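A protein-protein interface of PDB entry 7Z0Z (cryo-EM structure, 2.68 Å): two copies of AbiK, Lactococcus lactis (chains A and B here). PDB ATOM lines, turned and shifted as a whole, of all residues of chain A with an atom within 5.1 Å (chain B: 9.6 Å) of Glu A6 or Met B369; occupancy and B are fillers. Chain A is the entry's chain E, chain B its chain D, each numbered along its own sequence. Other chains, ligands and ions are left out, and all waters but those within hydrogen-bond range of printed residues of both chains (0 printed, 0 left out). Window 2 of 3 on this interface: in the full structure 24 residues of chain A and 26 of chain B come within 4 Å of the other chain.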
ATOM      1  N   SER A   2       0.465  -7.182 -16.842  1.00  0.00           N
ATOM      2  CA  SER A   2      -0.103  -8.510 -16.652  1.00  0.00           C
ATOM      3  C   SER A   2       0.560  -9.224 -15.482  1.00  0.00           C
ATOM      4  O   SER A   2       1.308  -8.617 -14.716  1.00  0.00           O
ATOM      5  CB  SER A   2       0.041  -9.339 -17.929  1.00  0.00           C
ATOM      6  OG  SER A   2       1.394  -9.699 -18.150  1.00  0.00           O
ATOM      7  N   MET A   3       0.268 -10.519 -15.343  1.00  0.00           N
ATOM      8  CA  MET A   3       0.941 -11.328 -14.334  1.00  0.00           C
ATOM      9  C   MET A   3       2.441 -11.375 -14.591  1.00  0.00           C
ATOM     10  O   MET A   3       3.255 -11.169 -13.681  1.00  0.00           O
ATOM     11  CB  MET A   3       0.363 -12.742 -14.340  1.00  0.00           C
ATOM     12  CG  MET A   3       1.044 -13.706 -13.392  1.00  0.00           C
ATOM     13  SD  MET A   3       0.043 -15.168 -13.066  1.00  0.00           S
ATOM     14  CE  MET A   3      -1.455 -14.429 -12.430  1.00  0.00           C
ATOM     15  N   LYS A   4       2.820 -11.634 -15.843  1.00  0.00           N
ATOM     16  CA  LYS A   4       4.221 -11.857 -16.169  1.00  0.00           C
ATOM     17  C   LYS A   4       5.032 -10.582 -15.997  1.00  0.00           C
ATOM     18  O   LYS A   4       6.168 -10.622 -15.520  1.00  0.00           O
ATOM     19  CB  LYS A   4       4.339 -12.388 -17.596  1.00  0.00           C
ATOM     20  CG  LYS A   4       3.626 -13.713 -17.801  1.00  0.00           C
ATOM     21  CD  LYS A   4       4.306 -14.829 -17.050  1.00  0.00           C
ATOM     22  CE  LYS A   4       3.598 -16.160 -17.239  1.00  0.00           C
ATOM     23  NZ  LYS A   4       3.718 -16.659 -18.634  1.00  0.00           N
ATOM     24  N   LYS A   5       4.461  -9.438 -16.381  1.00  0.00           N
ATOM     25  CA  LYS A   5       5.166  -8.172 -16.221  1.00  0.00           C
ATOM     26  C   LYS A   5       5.398  -7.846 -14.753  1.00  0.00           C
ATOM     27  O   LYS A   5       6.476  -7.373 -14.375  1.00  0.00           O
ATOM     28  CB  LYS A   5       4.385  -7.047 -16.898  1.00  0.00           C
ATOM     29  CG  LYS A   5       5.065  -5.694 -16.817  1.00  0.00           C
ATOM     30  CD  LYS A   5       4.315  -4.651 -17.626  1.00  0.00           C
ATOM     31  CE  LYS A   5       3.003  -4.275 -16.959  1.00  0.00           C
ATOM     32  NZ  LYS A   5       3.219  -3.536 -15.686  1.00  0.00           N
ATOM     33  N   GLU A   6       4.398  -8.090 -13.905  1.00  0.00           N
ATOM     34  CA  GLU A   6       4.553  -7.784 -12.489  1.00  0.00           C
ATOM     35  C   GLU A   6       5.568  -8.716 -11.837  1.00  0.00           C
ATOM     36  O   GLU A   6       6.393  -8.276 -11.025  1.00  0.00           O
ATOM     37  CB  GLU A   6       3.200  -7.869 -11.786  1.00  0.00           C
ATOM     38  CG  GLU A   6       2.215  -6.800 -12.216  1.00  0.00           C
ATOM     39  CD  GLU A   6       0.858  -6.957 -11.550  1.00  0.00           C
ATOM     40  OE1 GLU A   6       0.624  -8.001 -10.905  1.00  0.00           O
ATOM     41  OE2 GLU A   6       0.021  -6.039 -11.676  1.00  0.00           O
ATOM     42  N   PHE A   7       5.540 -10.000 -12.199  1.00  0.00           N
ATOM     43  CA  PHE A   7       6.561 -10.922 -11.707  1.00  0.00           C
ATOM     44  C   PHE A   7       7.950 -10.516 -12.180  1.00  0.00           C
ATOM     45  O   PHE A   7       8.923 -10.609 -11.423  1.00  0.00           O
ATOM     46  CB  PHE A   7       6.260 -12.350 -12.158  1.00  0.00           C
ATOM     47  CG  PHE A   7       5.079 -12.986 -11.486  1.00  0.00           C
ATOM     48  CD1 PHE A   7       4.139 -12.236 -10.813  1.00  0.00           C
ATOM     49  CD2 PHE A   7       4.913 -14.357 -11.545  1.00  0.00           C
ATOM     50  CE1 PHE A   7       3.064 -12.842 -10.210  1.00  0.00           C
ATOM     51  CE2 PHE A   7       3.837 -14.965 -10.943  1.00  0.00           C
ATOM     52  CZ  PHE A   7       2.910 -14.205 -10.273  1.00  0.00           C
ATOM     53  N   THR A   8       8.066 -10.089 -13.438  1.00  0.00           N
ATOM     54  CA  THR A   8       9.358  -9.674 -13.968  1.00  0.00           C
ATOM     55  C   THR A   8       9.879  -8.443 -13.243  1.00  0.00           C
ATOM     56  O   THR A   8      11.075  -8.351 -12.956  1.00  0.00           O
ATOM     57  CB  THR A   8       9.249  -9.409 -15.467  1.00  0.00           C
ATOM     58  OG1 THR A   8       8.831 -10.608 -16.131  1.00  0.00           O
ATOM     59  CG2 THR A   8      10.586  -8.972 -16.030  1.00  0.00           C
ATOM     60  N   GLU A   9       9.001  -7.490 -12.936  1.00  0.00           N
ATOM     61  CA  GLU A   9       9.423  -6.336 -12.151  1.00  0.00           C
ATOM     62  C   GLU A   9       9.899  -6.761 -10.769  1.00  0.00           C
ATOM     63  O   GLU A   9      10.948  -6.301 -10.293  1.00  0.00           O
ATOM     64  CB  GLU A   9       8.278  -5.333 -12.033  1.00  0.00           C
ATOM     65  CG  GLU A   9       7.954  -4.608 -13.323  1.00  0.00           C
ATOM     66  CD  GLU A   9       6.567  -4.001 -13.310  1.00  0.00           C
ATOM     67  OE1 GLU A   9       6.253  -3.214 -14.227  1.00  0.00           O
ATOM     68  OE2 GLU A   9       5.791  -4.311 -12.382  1.00  0.00           O
ATOM     69  N   LEU A  10       9.149  -7.653 -10.115  1.00  0.00           N
ATOM     70  CA  LEU A  10       9.543  -8.122  -8.791  1.00  0.00           C
ATOM     71  C   LEU A  10      10.924  -8.758  -8.820  1.00  0.00           C
ATOM     72  O   LEU A  10      11.798  -8.407  -8.023  1.00  0.00           O
ATOM     73  CB  LEU A  10       8.513  -9.113  -8.256  1.00  0.00           C
ATOM     74  CG  LEU A  10       8.926  -9.849  -6.982  1.00  0.00           C
ATOM     75  CD1 LEU A  10       8.872  -8.924  -5.787  1.00  0.00           C
ATOM     76  CD2 LEU A  10       8.052 -11.064  -6.759  1.00  0.00           C
ATOM     77  N   PHE A 142       3.930  -8.662  -2.454  1.00  0.00           N
ATOM     78  CA  PHE A 142       3.463 -10.042  -2.401  1.00  0.00           C
ATOM     79  C   PHE A 142       3.610 -10.561  -0.973  1.00  0.00           C
ATOM     80  O   PHE A 142       4.353 -11.495  -0.673  1.00  0.00           O
ATOM     81  CB  PHE A 142       4.223 -10.892  -3.404  1.00  0.00           C
ATOM     82  CG  PHE A 142       4.302 -10.290  -4.779  1.00  0.00           C
ATOM     83  CD1 PHE A 142       5.172  -9.250  -5.051  1.00  0.00           C
ATOM     84  CD2 PHE A 142       3.500 -10.759  -5.800  1.00  0.00           C
ATOM     85  CE1 PHE A 142       5.238  -8.695  -6.307  1.00  0.00           C
ATOM     86  CE2 PHE A 142       3.571 -10.210  -7.056  1.00  0.00           C
ATOM     87  CZ  PHE A 142       4.438  -9.178  -7.310  1.00  0.00           C
ATOM     88  N   ASP B 314     -11.379  -3.839  -2.574  1.00  0.00           N
ATOM     89  CA  ASP B 314     -10.455  -4.909  -2.213  1.00  0.00           C
ATOM     90  C   ASP B 314     -10.706  -5.391  -0.791  1.00  0.00           C
ATOM     91  O   ASP B 314     -10.635  -6.595  -0.513  1.00  0.00           O
ATOM     92  CB  ASP B 314      -9.017  -4.428  -2.376  1.00  0.00           C
ATOM     93  CG  ASP B 314      -8.639  -4.209  -3.824  1.00  0.00           C
ATOM     94  OD1 ASP B 314      -9.204  -4.899  -4.698  1.00  0.00           O
ATOM     95  OD2 ASP B 314      -7.784  -3.343  -4.093  1.00  0.00           O
ATOM     96  N   SER B 365     -16.840  -9.052 -10.102  1.00  0.00           N
ATOM     97  CA  SER B 365     -16.249  -9.290 -11.407  1.00  0.00           C
ATOM     98  C   SER B 365     -14.752  -9.044 -11.461  1.00  0.00           C
ATOM     99  O   SER B 365     -14.113  -9.469 -12.427  1.00  0.00           O
ATOM    100  CB  SER B 365     -16.926  -8.411 -12.465  1.00  0.00           C
ATOM    101  OG  SER B 365     -16.659  -7.044 -12.226  1.00  0.00           O
ATOM    102  N   LYS B 366     -14.182  -8.364 -10.468  1.00  0.00           N
ATOM    103  CA  LYS B 366     -12.751  -8.097 -10.473  1.00  0.00           C
ATOM    104  C   LYS B 366     -11.959  -9.393 -10.484  1.00  0.00           C
ATOM    105  O   LYS B 366     -12.191 -10.288  -9.669  1.00  0.00           O
ATOM    106  CB  LYS B 366     -12.353  -7.270  -9.255  1.00  0.00           C
ATOM    107  CG  LYS B 366     -10.887  -6.910  -9.222  1.00  0.00           C
ATOM    108  CD  LYS B 366     -10.560  -5.999  -8.060  1.00  0.00           C
ATOM    109  CE  LYS B 366      -9.063  -5.778  -7.963  1.00  0.00           C
ATOM    110  NZ  LYS B 366      -8.539  -5.029  -9.138  1.00  0.00           N
ATOM    111  N   ARG B 367     -11.014  -9.485 -11.408  1.00  0.00           N
ATOM    112  CA  ARG B 367     -10.071 -10.589 -11.469  1.00  0.00           C
ATOM    113  C   ARG B 367      -8.695 -10.034 -11.144  1.00  0.00           C
ATOM    114  O   ARG B 367      -8.168  -9.203 -11.890  1.00  0.00           O
ATOM    115  CB  ARG B 367     -10.085 -11.249 -12.845  1.00  0.00           C
ATOM    116  CG  ARG B 367      -9.001 -12.278 -13.041  1.00  0.00           C
ATOM    117  CD  ARG B 367      -9.405 -13.591 -12.420  1.00  0.00           C
ATOM    118  NE  ARG B 367     -10.566 -14.165 -13.085  1.00  0.00           N
ATOM    119  CZ  ARG B 367     -11.018 -15.392 -12.860  1.00  0.00           C
ATOM    120  NH1 ARG B 367     -10.409 -16.171 -11.982  1.00  0.00           N
ATOM    121  NH2 ARG B 367     -12.082 -15.837 -13.510  1.00  0.00           N
ATOM    122  N   ASN B 368      -8.125 -10.479 -10.031  1.00  0.00           N
ATOM    123  CA  ASN B 368      -6.840  -9.958  -9.599  1.00  0.00           C
ATOM    124  C   ASN B 368      -5.758 -10.379 -10.587  1.00  0.00           C
ATOM    125  O   ASN B 368      -5.654 -11.550 -10.955  1.00  0.00           O
ATOM    126  CB  ASN B 368      -6.521 -10.459  -8.194  1.00  0.00           C
ATOM    127  CG  ASN B 368      -5.257  -9.860  -7.632  1.00  0.00           C
ATOM    128  OD1 ASN B 368      -4.184  -9.993  -8.208  1.00  0.00           O
ATOM    129  ND2 ASN B 368      -5.378  -9.198  -6.490  1.00  0.00           N
ATOM    130  N   MET B 369      -4.952  -9.412 -11.021  1.00  0.00           N
ATOM    131  CA  MET B 369      -4.031  -9.662 -12.125  1.00  0.00           C
ATOM    132  C   MET B 369      -2.889 -10.583 -11.712  1.00  0.00           C
ATOM    133  O   MET B 369      -2.338 -11.307 -12.550  1.00  0.00           O
ATOM    134  CB  MET B 369      -3.489  -8.336 -12.659  1.00  0.00           C
ATOM    135  CG  MET B 369      -2.491  -7.660 -11.741  1.00  0.00           C
ATOM    136  SD  MET B 369      -3.264  -7.057 -10.228  1.00  0.00           S
ATOM    137  CE  MET B 369      -4.272  -5.728 -10.872  1.00  0.00           C
ATOM    138  N   VAL B 370      -2.521 -10.578 -10.436  1.00  0.00           N
ATOM    139  CA  VAL B 370      -1.364 -11.346  -9.991  1.00  0.00           C
ATOM    140  C   VAL B 370      -1.771 -12.638  -9.288  1.00  0.00           C
ATOM    141  O   VAL B 370      -1.170 -13.688  -9.523  1.00  0.00           O
ATOM    142  CB  VAL B 370      -0.453 -10.463  -9.113  1.00  0.00           C
ATOM    143  CG1 VAL B 370      -1.142 -10.047  -7.840  1.00  0.00           C
ATOM    144  CG2 VAL B 370       0.796 -11.209  -8.771  1.00  0.00           C
ATOM    145  N   THR B 371      -2.779 -12.610  -8.418  1.00  0.00           N
ATOM    146  CA  THR B 371      -3.231 -13.836  -7.777  1.00  0.00           C
ATOM    147  C   THR B 371      -4.237 -14.605  -8.619  1.00  0.00           C
ATOM    148  O   THR B 371      -4.498 -15.778  -8.325  1.00  0.00           O
ATOM    149  CB  THR B 371      -3.845 -13.531  -6.410  1.00  0.00           C
ATOM    150  OG1 THR B 371      -5.095 -12.856  -6.580  1.00  0.00           O
ATOM    151  CG2 THR B 371      -2.914 -12.652  -5.599  1.00  0.00           C
ATOM    152  N   ASN B 372      -4.783 -13.978  -9.662  1.00  0.00           N
ATOM    153  CA  ASN B 372      -5.763 -14.601 -10.553  1.00  0.00           C
ATOM    154  C   ASN B 372      -6.973 -15.087  -9.752  1.00  0.00           C
ATOM    155  O   ASN B 372      -7.512 -16.168  -9.987  1.00  0.00           O
ATOM    156  CB  ASN B 372      -5.118 -15.735 -11.356  1.00  0.00           C
ATOM    157  CG  ASN B 372      -6.015 -16.273 -12.454  1.00  0.00           C
ATOM    158  OD1 ASN B 372      -7.147 -15.830 -12.628  1.00  0.00           O
ATOM    159  ND2 ASN B 372      -5.503 -17.238 -13.207  1.00  0.00           N
ATOM    160  N   PHE B 373      -7.395 -14.280  -8.784  1.00  0.00           N
ATOM    161  CA  PHE B 373      -8.447 -14.641  -7.843  1.00  0.00           C
ATOM    162  C   PHE B 373      -9.695 -13.818  -8.110  1.00  0.00           C
ATOM    163  O   PHE B 373      -9.630 -12.587  -8.187  1.00  0.00           O
ATOM    164  CB  PHE B 373      -7.977 -14.430  -6.403  1.00  0.00           C
ATOM    165  CG  PHE B 373      -9.058 -14.608  -5.378  1.00  0.00           C
ATOM    166  CD1 PHE B 373      -9.434 -15.868  -4.960  1.00  0.00           C
ATOM    167  CD2 PHE B 373      -9.686 -13.510  -4.823  1.00  0.00           C
ATOM    168  CE1 PHE B 373     -10.418 -16.027  -4.018  1.00  0.00           C
ATOM    169  CE2 PHE B 373     -10.673 -13.667  -3.881  1.00  0.00           C
ATOM    170  CZ  PHE B 373     -11.039 -14.926  -3.479  1.00  0.00           C
ATOM    171  N   ASN B 374     -10.831 -14.495  -8.244  1.00  0.00           N
ATOM    172  CA  ASN B 374     -12.124 -13.842  -8.348  1.00  0.00           C
ATOM    173  C   ASN B 374     -13.032 -14.424  -7.275  1.00  0.00           C
ATOM    174  O   ASN B 374     -13.067 -15.640  -7.079  1.00  0.00           O
ATOM    175  CB  ASN B 374     -12.724 -14.032  -9.744  1.00  0.00           C
ATOM    176  CG  ASN B 374     -14.053 -13.344  -9.907  1.00  0.00           C
ATOM    177  OD1 ASN B 374     -15.036 -13.698  -9.268  1.00  0.00           O
ATOM    178  ND2 ASN B 374     -14.089 -12.344 -10.769  1.00  0.00           N
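CE of Met A3 touches O of Met B369, at 3.2 Å.
Met A3 touches Val B370.
OE1 of Glu A6 touches CB of Val B370 (3.2 Å).
Phe A7 touches Val B370 (CE1 to CG2, 3.1 Å).
Val B370 touches Phe A142.
SD of Met B369 sits close to OE2 of Glu A6, 3.7 Å away.
Met B369 touches just these residues of chain A: Met A3 (3.2 Å) and Glu A6 (3.0 Å).
Met A3 touches just these residues of chain B: Met B369 (3.2 Å) and Val B370 (3.0 Å).
Of the printed residues of chain B, Phe A7 touches Val B370 (3.1 Å).
Of the printed residues of chain A, Val B370 touches Met A3 (3.0 Å), Glu A6 (3.2 Å), Phe A7 (3.1 Å) and Phe A142 (3.4 Å).
Of the printed residues of chain B, Phe A142 touches Val B370.
Asn B368 touches none of the printed residues of chain A.
The nearest residue of chain B that does not touch Glu A6 is Asn B368 (5.9 Å).
The nearest printed residue of chain B that does not touch Phe A7 is Met B369 (6.1 Å).
SD of Met B369 sits close to OD1 of Asn B368 (3.7 Å).
The backbone NH (N) of Val B370 is in hydrogen-bond range of the side-chain amide oxygen (OD1) of Asn B368, at 2.8 Å.
No position is printed for both chains.
Of the 6 pairs that touch across the chains among the printed residues, none has its exchanged pair printed and touching as well.
Of the 11 printed residues of chain B, 2 touch a printed residue of chain A.
Printed residues of chain B that touch a printed residue of chain A: Met B369 and Val B370.
Printed residues of chain A that touch a printed residue of chain B: Met A3, Glu A6, Phe A7 and Phe A142.
Hydrophobic or aromatic side chains of chain A that line the printed part of chain B: Met A3, Phe A7 and Phe A142.
Among the printed residues, 6 pairs touch across the chains.
Among the printed residues, no Asp or Glu carboxylate lies within 4 Å of a Lys or Arg side-chain nitrogen of the other chain.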
